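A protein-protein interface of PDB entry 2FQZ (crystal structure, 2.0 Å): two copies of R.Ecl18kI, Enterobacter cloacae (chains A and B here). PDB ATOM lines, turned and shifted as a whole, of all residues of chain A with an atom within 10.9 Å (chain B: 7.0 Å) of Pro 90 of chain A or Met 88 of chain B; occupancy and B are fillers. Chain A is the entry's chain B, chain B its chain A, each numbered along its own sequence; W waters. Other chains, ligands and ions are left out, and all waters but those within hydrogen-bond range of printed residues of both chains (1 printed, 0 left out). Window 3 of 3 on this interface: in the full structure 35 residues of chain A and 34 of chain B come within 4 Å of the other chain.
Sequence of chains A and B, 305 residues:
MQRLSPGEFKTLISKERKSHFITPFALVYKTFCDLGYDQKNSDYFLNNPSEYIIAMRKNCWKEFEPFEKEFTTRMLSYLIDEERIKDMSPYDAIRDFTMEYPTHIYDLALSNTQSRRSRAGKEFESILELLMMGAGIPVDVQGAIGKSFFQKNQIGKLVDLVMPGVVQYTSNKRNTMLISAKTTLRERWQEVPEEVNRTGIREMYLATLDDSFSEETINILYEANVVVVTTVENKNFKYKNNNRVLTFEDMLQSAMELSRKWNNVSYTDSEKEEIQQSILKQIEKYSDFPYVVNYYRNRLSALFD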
ATOM      1  N   ILE A  80      20.295  11.490  18.779  1.00  0.00           N
ATOM      2  CA  ILE A  80      20.227  11.717  20.214  1.00  0.00           C
ATOM      3  C   ILE A  80      19.407  10.555  20.769  1.00  0.00           C
ATOM      4  O   ILE A  80      18.405  10.143  20.170  1.00  0.00           O
ATOM      5  CB  ILE A  80      19.611  13.089  20.588  1.00  0.00           C
ATOM      6  CG1 ILE A  80      20.438  14.224  19.971  1.00  0.00           C
ATOM      7  CG2 ILE A  80      19.543  13.255  22.112  1.00  0.00           C
ATOM      8  CD1 ILE A  80      19.792  15.610  20.057  1.00  0.00           C
ATOM      9  N   GLU A  82      17.534   9.554  23.939  1.00  0.00           N
ATOM     10  CA  GLU A  82      16.946   9.922  25.223  1.00  0.00           C
ATOM     11  C   GLU A  82      17.070   8.785  26.242  1.00  0.00           C
ATOM     12  O   GLU A  82      17.380   9.034  27.407  1.00  0.00           O
ATOM     13  CB  GLU A  82      15.492  10.395  25.068  1.00  0.00           C
ATOM     14  CG  GLU A  82      14.740  10.643  26.393  1.00  0.00           C
ATOM     15  CD  GLU A  82      15.333  11.770  27.245  1.00  0.00           C
ATOM     16  OE1 GLU A  82      14.907  12.934  27.080  1.00  0.00           O
ATOM     17  OE2 GLU A  82      16.201  11.488  28.100  1.00  0.00           O
ATOM     18  N   ILE A  85      20.715   8.482  27.583  1.00  0.00           N
ATOM     19  CA  ILE A  85      21.156   9.640  28.354  1.00  0.00           C
ATOM     20  C   ILE A  85      20.146  10.013  29.451  1.00  0.00           C
ATOM     21  O   ILE A  85      19.848  11.188  29.683  1.00  0.00           O
ATOM     22  CB  ILE A  85      21.486  10.827  27.396  1.00  0.00           C
ATOM     23  CG1 ILE A  85      22.251  10.308  26.171  1.00  0.00           C
ATOM     24  CG2 ILE A  85      22.255  11.925  28.120  1.00  0.00           C
ATOM     25  CD1 ILE A  85      23.297  11.238  25.628  1.00  0.00           C
ATOM     26  N   LYS A  86      19.641   8.990  30.135  1.00  0.00           N
ATOM     27  CA  LYS A  86      18.614   9.153  31.162  1.00  0.00           C
ATOM     28  C   LYS A  86      19.086  10.005  32.337  1.00  0.00           C
ATOM     29  O   LYS A  86      18.597  11.122  32.557  1.00  0.00           O
ATOM     30  CB  LYS A  86      18.158   7.780  31.677  1.00  0.00           C
ATOM     31  CG  LYS A  86      17.156   7.046  30.794  1.00  0.00           C
ATOM     32  CD  LYS A  86      15.703   7.366  31.168  1.00  0.00           C
ATOM     33  CE  LYS A  86      15.267   8.754  30.693  1.00  0.00           C
ATOM     34  NZ  LYS A  86      15.576   8.984  29.254  1.00  0.00           N
ATOM     35  N   ASP A  87      20.038   9.452  33.084  1.00  0.00           N
ATOM     36  CA  ASP A  87      20.511  10.029  34.334  1.00  0.00           C
ATOM     37  C   ASP A  87      21.954  10.500  34.229  1.00  0.00           C
ATOM     38  O   ASP A  87      22.741  10.371  35.179  1.00  0.00           O
ATOM     39  CB  ASP A  87      20.364   9.011  35.468  1.00  0.00           C
ATOM     40  CG  ASP A  87      18.925   8.850  35.927  1.00  0.00           C
ATOM     41  OD1 ASP A  87      18.017   9.461  35.321  1.00  0.00           O
ATOM     42  OD2 ASP A  87      18.702   8.107  36.908  1.00  0.00           O
ATOM     43  N   MET A  88      22.289  11.036  33.049  1.00  0.00           N
ATOM     44  CA  MET A  88      23.551  11.728  32.875  1.00  0.00           C
ATOM     45  C   MET A  88      23.356  13.193  33.239  1.00  0.00           C
ATOM     46  O   MET A  88      22.240  13.758  33.094  1.00  0.00           O
ATOM     47  CB  MET A  88      24.032  11.628  31.425  1.00  0.00           C
ATOM     48  CG  MET A  88      24.382  10.222  30.961  1.00  0.00           C
ATOM     49  SD  MET A  88      25.225  10.277  29.365  1.00  0.00           S
ATOM     50  CE  MET A  88      25.166   8.546  28.888  1.00  0.00           C
ATOM     51  N   SER A  89      24.443  13.794  33.731  1.00  0.00           N
ATOM     52  CA  SER A  89      24.541  15.241  33.855  1.00  0.00           C
ATOM     53  C   SER A  89      24.654  15.852  32.459  1.00  0.00           C
ATOM     54  O   SER A  89      25.153  15.191  31.540  1.00  0.00           O
ATOM     55  CB  SER A  89      25.785  15.608  34.668  1.00  0.00           C
ATOM     56  OG  SER A  89      26.977  15.207  33.991  1.00  0.00           O
ATOM     57  N   PRO A  90      24.192  17.106  32.289  1.00  0.00           N
ATOM     58  CA  PRO A  90      24.378  17.792  31.007  1.00  0.00           C
ATOM     59  C   PRO A  90      25.804  17.717  30.460  1.00  0.00           C
ATOM     60  O   PRO A  90      25.977  17.550  29.251  1.00  0.00           O
ATOM     61  CB  PRO A  90      24.004  19.248  31.320  1.00  0.00           C
ATOM     62  CG  PRO A  90      23.791  19.313  32.798  1.00  0.00           C
ATOM     63  CD  PRO A  90      23.440  17.942  33.235  1.00  0.00           C
ATOM     64  N   TYR A  91      26.811  17.825  31.329  1.00  0.00           N
ATOM     65  CA  TYR A  91      28.204  17.725  30.884  1.00  0.00           C
ATOM     66  C   TYR A  91      28.552  16.320  30.376  1.00  0.00           C
ATOM     67  O   TYR A  91      29.211  16.179  29.337  1.00  0.00           O
ATOM     68  CB  TYR A  91      29.182  18.188  31.971  1.00  0.00           C
ATOM     69  CG  TYR A  91      30.617  17.821  31.670  1.00  0.00           C
ATOM     70  CD1 TYR A  91      31.407  18.612  30.832  1.00  0.00           C
ATOM     71  CD2 TYR A  91      31.179  16.663  32.207  1.00  0.00           C
ATOM     72  CE1 TYR A  91      32.726  18.258  30.549  1.00  0.00           C
ATOM     73  CE2 TYR A  91      32.485  16.304  31.927  1.00  0.00           C
ATOM     74  CZ  TYR A  91      33.253  17.101  31.102  1.00  0.00           C
ATOM     75  OH  TYR A  91      34.550  16.723  30.846  1.00  0.00           O
ATOM     76  N   ASP A  92      28.110  15.295  31.109  1.00  0.00           N
ATOM     77  CA  ASP A  92      28.317  13.896  30.706  1.00  0.00           C
ATOM     78  C   ASP A  92      27.461  13.526  29.489  1.00  0.00           C
ATOM     79  O   ASP A  92      27.860  12.685  28.678  1.00  0.00           O
ATOM     80  CB  ASP A  92      28.043  12.925  31.867  1.00  0.00           C
ATOM     81  CG  ASP A  92      28.953  13.161  33.070  1.00  0.00           C
ATOM     82  OD1 ASP A  92      30.094  13.633  32.877  1.00  0.00           O
ATOM     83  OD2 ASP A  92      28.526  12.867  34.213  1.00  0.00           O
ATOM     84  N   ALA A  93      26.290  14.152  29.370  1.00  0.00           N
ATOM     85  CA  ALA A  93      25.434  13.999  28.191  1.00  0.00           C
ATOM     86  C   ALA A  93      26.140  14.447  26.895  1.00  0.00           C
ATOM     87  O   ALA A  93      26.225  13.693  25.912  1.00  0.00           O
ATOM     88  CB  ALA A  93      24.148  14.777  28.383  1.00  0.00           C
ATOM     89  N   ILE A  94      26.642  15.680  26.915  1.00  0.00           N
ATOM     90  CA  ILE A  94      27.433  16.238  25.827  1.00  0.00           C
ATOM     91  C   ILE A  94      28.715  15.424  25.637  1.00  0.00           C
ATOM     92  O   ILE A  94      29.114  15.137  24.499  1.00  0.00           O
ATOM     93  CB  ILE A  94      27.757  17.743  26.071  1.00  0.00           C
ATOM     94  CG1 ILE A  94      26.456  18.532  26.347  1.00  0.00           C
ATOM     95  CG2 ILE A  94      28.549  18.316  24.892  1.00  0.00           C
ATOM     96  CD1 ILE A  94      26.603  20.054  26.477  1.00  0.00           C
ATOM     97  N   ARG A  95      29.342  15.053  26.752  1.00  0.00           N
ATOM     98  CA  ARG A  95      30.536  14.214  26.743  1.00  0.00           C
ATOM     99  C   ARG A  95      30.295  12.923  25.963  1.00  0.00           C
ATOM    100  O   ARG A  95      31.039  12.622  25.033  1.00  0.00           O
ATOM    101  N   ASP A  96      29.239  12.193  26.322  1.00  0.00           N
ATOM    102  CA  ASP A  96      28.839  10.976  25.612  1.00  0.00           C
ATOM    103  C   ASP A  96      28.660  11.193  24.120  1.00  0.00           C
ATOM    104  O   ASP A  96      29.128  10.401  23.313  1.00  0.00           O
ATOM    105  CB  ASP A  96      27.523  10.439  26.170  1.00  0.00           C
ATOM    106  CG  ASP A  96      27.083   9.154  25.490  1.00  0.00           C
ATOM    107  OD1 ASP A  96      27.711   8.106  25.738  1.00  0.00           O
ATOM    108  OD2 ASP A  96      26.104   9.186  24.715  1.00  0.00           O
ATOM    109  N   PHE A  97      27.956  12.264  23.769  1.00  0.00           N
ATOM    110  CA  PHE A  97      27.633  12.560  22.386  1.00  0.00           C
ATOM    111  C   PHE A  97      28.898  12.704  21.548  1.00  0.00           C
ATOM    112  O   PHE A  97      29.005  12.125  20.462  1.00  0.00           O
ATOM    113  CB  PHE A  97      26.801  13.831  22.321  1.00  0.00           C
ATOM    114  CG  PHE A  97      26.133  14.050  21.001  1.00  0.00           C
ATOM    115  CD1 PHE A  97      24.903  13.456  20.728  1.00  0.00           C
ATOM    116  CD2 PHE A  97      26.714  14.867  20.037  1.00  0.00           C
ATOM    117  CE1 PHE A  97      24.271  13.667  19.513  1.00  0.00           C
ATOM    118  CE2 PHE A  97      26.086  15.081  18.821  1.00  0.00           C
ATOM    119  CZ  PHE A  97      24.862  14.482  18.560  1.00  0.00           C
ATOM    120  N   THR A  98      29.857  13.466  22.074  1.00  0.00           N
ATOM    121  CA  THR A  98      31.140  13.669  21.407  1.00  0.00           C
ATOM    122  C   THR A  98      31.967  12.382  21.339  1.00  0.00           C
ATOM    123  O   THR A  98      32.940  12.315  20.585  1.00  0.00           O
ATOM    124  CB  THR A  98      32.001  14.806  22.060  1.00  0.00           C
ATOM    125  OG1 THR A  98      32.609  14.325  23.295  1.00  0.00           O
ATOM    126  CG2 THR A  98      31.115  16.088  22.326  1.00  0.00           C
ATOM    127  N   ILE B  80      32.368  22.523  25.127  1.00  0.00           N
ATOM    128  CA  ILE B  80      31.470  22.245  26.254  1.00  0.00           C
ATOM    129  C   ILE B  80      31.600  23.326  27.315  1.00  0.00           C
ATOM    130  O   ILE B  80      32.678  23.563  27.867  1.00  0.00           O
ATOM    131  CB  ILE B  80      31.673  20.836  26.875  1.00  0.00           C
ATOM    132  CG1 ILE B  80      31.817  19.767  25.779  1.00  0.00           C
ATOM    133  CG2 ILE B  80      30.508  20.500  27.800  1.00  0.00           C
ATOM    134  CD1 ILE B  80      32.105  18.357  26.294  1.00  0.00           C
ATOM    135  N   GLU B  82      30.406  24.410  30.709  1.00  0.00           N
ATOM    136  CA  GLU B  82      29.870  23.862  31.954  1.00  0.00           C
ATOM    137  C   GLU B  82      28.812  24.771  32.560  1.00  0.00           C
ATOM    138  O   GLU B  82      27.811  24.289  33.101  1.00  0.00           O
ATOM    139  CB  GLU B  82      30.995  23.653  32.973  1.00  0.00           C
ATOM    140  N   ARG B  84      27.031  27.226  30.934  1.00  0.00           N
ATOM    141  CA  ARG B  84      25.884  27.320  30.033  1.00  0.00           C
ATOM    142  C   ARG B  84      24.896  26.172  30.250  1.00  0.00           C
ATOM    143  O   ARG B  84      23.675  26.376  30.225  1.00  0.00           O
ATOM    144  CB  ARG B  84      26.354  27.336  28.571  1.00  0.00           C
ATOM    145  CG  ARG B  84      25.231  27.377  27.552  1.00  0.00           C
ATOM    146  CD  ARG B  84      25.711  27.877  26.201  1.00  0.00           C
ATOM    147  NE  ARG B  84      24.667  28.681  25.568  1.00  0.00           N
ATOM    148  CZ  ARG B  84      24.874  29.582  24.613  1.00  0.00           C
ATOM    149  NH1 ARG B  84      26.102  29.815  24.157  1.00  0.00           N
ATOM    150  NH2 ARG B  84      23.849  30.259  24.116  1.00  0.00           N
ATOM    151  N   ILE B  85      25.429  24.973  30.471  1.00  0.00           N
ATOM    152  CA  ILE B  85      24.631  23.749  30.443  1.00  0.00           C
ATOM    153  C   ILE B  85      24.262  23.199  31.823  1.00  0.00           C
ATOM    154  O   ILE B  85      23.400  22.328  31.917  1.00  0.00           O
ATOM    155  CB  ILE B  85      25.322  22.639  29.602  1.00  0.00           C
ATOM    156  CG1 ILE B  85      26.603  22.157  30.297  1.00  0.00           C
ATOM    157  CG2 ILE B  85      25.584  23.143  28.180  1.00  0.00           C
ATOM    158  CD1 ILE B  85      27.214  20.879  29.728  1.00  0.00           C
ATOM    159  N   LYS B  86      24.909  23.698  32.880  1.00  0.00           N
ATOM    160  CA  LYS B  86      24.571  23.298  34.261  1.00  0.00           C
ATOM    161  C   LYS B  86      23.093  23.566  34.543  1.00  0.00           C
ATOM    162  O   LYS B  86      22.592  24.665  34.280  1.00  0.00           O
ATOM    163  CB  LYS B  86      25.464  24.002  35.298  1.00  0.00           C
ATOM    164  CG  LYS B  86      25.130  25.494  35.521  1.00  0.00           C
ATOM    165  CD  LYS B  86      25.925  26.076  36.691  1.00  0.00           C
ATOM    166  CE  LYS B  86      25.729  27.590  36.763  1.00  0.00           C
ATOM    167  NZ  LYS B  86      26.251  28.182  38.025  1.00  0.00           N
ATOM    168  N   ASP B  87      22.401  22.547  35.046  1.00  0.00           N
ATOM    169  CA  ASP B  87      20.942  22.592  35.286  1.00  0.00           C
ATOM    170  C   ASP B  87      20.061  22.386  34.044  1.00  0.00           C
ATOM    171  O   ASP B  87      18.835  22.303  34.166  1.00  0.00           O
ATOM    172  CB  ASP B  87      20.510  23.850  36.069  1.00  0.00           C
ATOM    173  N   MET B  88      20.667  22.304  32.860  1.00  0.00           N
ATOM    174  CA  MET B  88      19.932  21.864  31.676  1.00  0.00           C
ATOM    175  C   MET B  88      19.619  20.380  31.797  1.00  0.00           C
ATOM    176  O   MET B  88      20.366  19.628  32.438  1.00  0.00           O
ATOM    177  CB  MET B  88      20.751  22.079  30.401  1.00  0.00           C
ATOM    178  CG  MET B  88      20.654  23.458  29.787  1.00  0.00           C
ATOM    179  SD  MET B  88      21.561  23.481  28.225  1.00  0.00           S
ATOM    180  CE  MET B  88      21.190  25.132  27.632  1.00  0.00           C
ATOM    181  N   SER B  89      18.520  19.960  31.177  1.00  0.00           N
ATOM    182  CA  SER B  89      18.286  18.545  30.943  1.00  0.00           C
ATOM    183  C   SER B  89      19.407  18.069  30.021  1.00  0.00           C
ATOM    184  O   SER B  89      19.784  18.788  29.100  1.00  0.00           O
ATOM    185  CB  SER B  89      16.924  18.318  30.289  1.00  0.00           C
ATOM    186  OG  SER B  89      16.656  16.915  30.175  1.00  0.00           O
ATOM    187  N   PRO B  90      19.982  16.886  30.301  1.00  0.00           N
ATOM    188  CA  PRO B  90      21.027  16.296  29.456  1.00  0.00           C
ATOM    189  C   PRO B  90      20.663  16.255  27.966  1.00  0.00           C
ATOM    190  O   PRO B  90      21.489  16.622  27.117  1.00  0.00           O
ATOM    191  CB  PRO B  90      21.174  14.870  30.012  1.00  0.00           C
ATOM    192  CG  PRO B  90      20.036  14.682  31.006  1.00  0.00           C
ATOM    193  CD  PRO B  90      19.693  16.050  31.481  1.00  0.00           C
ATOM    194  N   TYR B  91      19.443  15.811  27.656  1.00  0.00           N
ATOM    195  CA  TYR B  91      18.952  15.851  26.282  1.00  0.00           C
ATOM    196  C   TYR B  91      18.936  17.289  25.773  1.00  0.00           C
ATOM    197  O   TYR B  91      19.372  17.554  24.654  1.00  0.00           O
ATOM    198  CB  TYR B  91      17.562  15.216  26.160  1.00  0.00           C
ATOM    199  CG  TYR B  91      16.782  15.693  24.954  1.00  0.00           C
ATOM    200  CD1 TYR B  91      17.002  15.146  23.686  1.00  0.00           C
ATOM    201  CD2 TYR B  91      15.837  16.705  25.079  1.00  0.00           C
ATOM    202  CE1 TYR B  91      16.290  15.595  22.578  1.00  0.00           C
ATOM    203  CE2 TYR B  91      15.121  17.164  23.983  1.00  0.00           C
ATOM    204  CZ  TYR B  91      15.348  16.607  22.737  1.00  0.00           C
ATOM    205  OH  TYR B  91      14.629  17.069  21.658  1.00  0.00           O
ATOM    206  N   ASP B  92      18.439  18.205  26.603  1.00  0.00           N
ATOM    207  CA  ASP B  92      18.431  19.631  26.282  1.00  0.00           C
ATOM    208  C   ASP B  92      19.842  20.208  26.104  1.00  0.00           C
ATOM    209  O   ASP B  92      20.053  21.064  25.238  1.00  0.00           O
ATOM    210  CB  ASP B  92      17.642  20.429  27.329  1.00  0.00           C
ATOM    211  CG  ASP B  92      16.127  20.345  27.121  1.00  0.00           C
ATOM    212  OD1 ASP B  92      15.683  19.739  26.118  1.00  0.00           O
ATOM    213  OD2 ASP B  92      15.376  20.893  27.960  1.00  0.00           O
ATOM    214  N   ALA B  93      20.798  19.734  26.906  1.00  0.00           N
ATOM    215  CA  ALA B  93      22.204  20.135  26.771  1.00  0.00           C
ATOM    216  C   ALA B  93      22.797  19.656  25.444  1.00  0.00           C
ATOM    217  O   ALA B  93      23.637  20.340  24.854  1.00  0.00           O
ATOM    218  CB  ALA B  93      23.024  19.623  27.936  1.00  0.00           C
ATOM    219  N   ILE B  94      22.340  18.492  24.987  1.00  0.00           N
ATOM    220  CA  ILE B  94      22.733  17.963  23.685  1.00  0.00           C
ATOM    221  C   ILE B  94      22.070  18.732  22.541  1.00  0.00           C
ATOM    222  O   ILE B  94      22.741  19.084  21.567  1.00  0.00           O
ATOM    223  CB  ILE B  94      22.482  16.439  23.560  1.00  0.00           C
ATOM    224  CG1 ILE B  94      23.305  15.680  24.608  1.00  0.00           C
ATOM    225  CG2 ILE B  94      22.845  15.952  22.157  1.00  0.00           C
ATOM    226  CD1 ILE B  94      23.116  14.170  24.565  1.00  0.00           C
ATOM    227  N   ASP B  96      21.066  21.835  22.725  1.00  0.00           N
ATOM    228  CA  ASP B  96      21.833  23.089  22.785  1.00  0.00           C
ATOM    229  C   ASP B  96      23.152  22.964  22.027  1.00  0.00           C
ATOM    230  O   ASP B  96      23.451  23.785  21.170  1.00  0.00           O
ATOM    231  CB  ASP B  96      22.114  23.522  24.229  1.00  0.00           C
ATOM    232  CG  ASP B  96      22.833  24.871  24.313  1.00  0.00           C
ATOM    233  OD1 ASP B  96      22.254  25.897  23.889  1.00  0.00           O
ATOM    234  OD2 ASP B  96      23.977  24.902  24.826  1.00  0.00           O
ATOM    235  N   PHE B  97      23.920  21.928  22.358  1.00  0.00           N
ATOM    236  CA  PHE B  97      25.227  21.678  21.747  1.00  0.00           C
ATOM    237  C   PHE B  97      25.109  21.502  20.231  1.00  0.00           C
ATOM    238  O   PHE B  97      25.898  22.087  19.495  1.00  0.00           O
ATOM    239  CB  PHE B  97      25.889  20.455  22.403  1.00  0.00           C
ATOM    240  CG  PHE B  97      27.350  20.287  22.075  1.00  0.00           C
ATOM    241  CD1 PHE B  97      28.326  21.000  22.774  1.00  0.00           C
ATOM    242  CD2 PHE B  97      27.756  19.387  21.092  1.00  0.00           C
ATOM    243  CE1 PHE B  97      29.684  20.830  22.486  1.00  0.00           C
ATOM    244  CE2 PHE B  97      29.108  19.212  20.798  1.00  0.00           C
ATOM    245  CZ  PHE B  97      30.073  19.936  21.492  1.00  0.00           C
HETATM  246  O   HOH W   1      19.331  13.106  27.764  1.00  0.00           O
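Water W1 bridges the backbone NH (N) of Tyr 91 of chain B (2.7 Å) and the backbone carbonyl oxygen (O) of Ile 85 of chain A (2.8 Å).
The side-chain amino group (NZ) of Lys 86 of chain A lies within salt-bridge range of the side-chain carboxylate (OE2) of Glu 82 of chain A (2.8 Å).
Of the printed residues of chain B, Ile 80 of chain A touches Tyr 91 and Ile 94. Lys 86 of chain A touches none of the printed residues of chain B. Ser 89 of chain A touches none of the printed residues of chain B. Printed residues of chain B within 4 Å of Pro 90 of chain A: Ile 85, Met 88, Pro 90 and Ala 93. Printed residues of chain B within 4 Å of Phe 97 of chain A: Ile 94. Printed residues of chain A within 4 Å of Ile 80 of chain B: Tyr 91 and Ile 94. Ile 85 of chain B touches just these residues of chain A: Pro 90 (3.2 Å), Tyr 91 (3.5 Å) and Ile 94 (3.4 Å). No residue of chain A comes within 4 Å of Asp 87 of chain B. No residue of chain A comes within 4 Å of Ser 89 of chain B. Of the printed residues of chain A, Pro 90 of chain B touches Ile 85, Met 88, Pro 90 and Ala 93. Of chain A, only Pro 90 (3.5 Å) and Ile 94 (3.4 Å) come within 4 Å of Ala 93 of chain B. The nearest residue of chain A that does not touch Met 88 of chain B is Ser 89 of chain A (5.7 Å).
Glu 82 of chain A touches Tyr 91 of chain B, but with the chains exchanged Tyr 91 of chain A does not touch Glu 82 of chain B (5.5 Å). Met 88 of chain A touches Pro 90 of chain B, and with the chains exchanged Pro 90 of chain A touches Met 88 of chain B. Pro 90 of chain A touches Ala 93 of chain B, and with the chains exchanged Ala 93 of chain A touches Pro 90 of chain B. Tyr 91 of chain A touches Ile 85 of chain B, but with the chains exchanged Ile 85 of chain A does not touch Tyr 91 of chain B (4.8 Å). 14 positions are printed for both chains. Of the 19 pairs that touch across the chains among the printed residues, 17 have their exchanged pair printed and touching as well.
Of the 15 printed residues of chain B, 8 touch a printed residue of chain A. Hydrophobic or aromatic side chains of chain B within 4 Å of the printed part of chain A: Ile 80, Ile 85, Pro 90, Tyr 91, Ala 93, Ile 94 and Phe 97. Of the 16 printed residues of chain A, 9 touch a printed residue of chain B. Hydrophobic or aromatic side chains of chain A that line the printed part of chain B: Ile 80, Ile 85, Pro 90, Tyr 91, Ala 93, Ile 94 and Phe 97.
CG2 of Ile 80 of chain A touches CD1 of Tyr 91 of chain B, at 3.5 Å. CB of Tyr 91 of chain B touches OE1 of Glu 82 of chain A, at 3.6 Å. Pro 90 of chain B touches Ile 85 of chain A (CB to CG2, 3.7 Å). CG of Pro 90 of chain A touches O of Met 88 of chain B (3.5 Å). Pro 90 of chain B touches Pro 90 of chain A. Tyr 91 of chain A touches Ile 80 of chain B (CD1 to CG2, 3.7 Å). Tyr 91 of chain A touches Ile 85 of chain B (N to CD1, 3.5 Å). Ile 94 of chain A touches Ile 85 of chain B (CD1 to CD1, 3.4 Å). CD1 of Ile 94 of chain A touches O of Ala 93 of chain B, at 3.4 Å. Ile 94 of chain B touches Phe 97 of chain A (CG2 to CD1, 3.5 Å).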
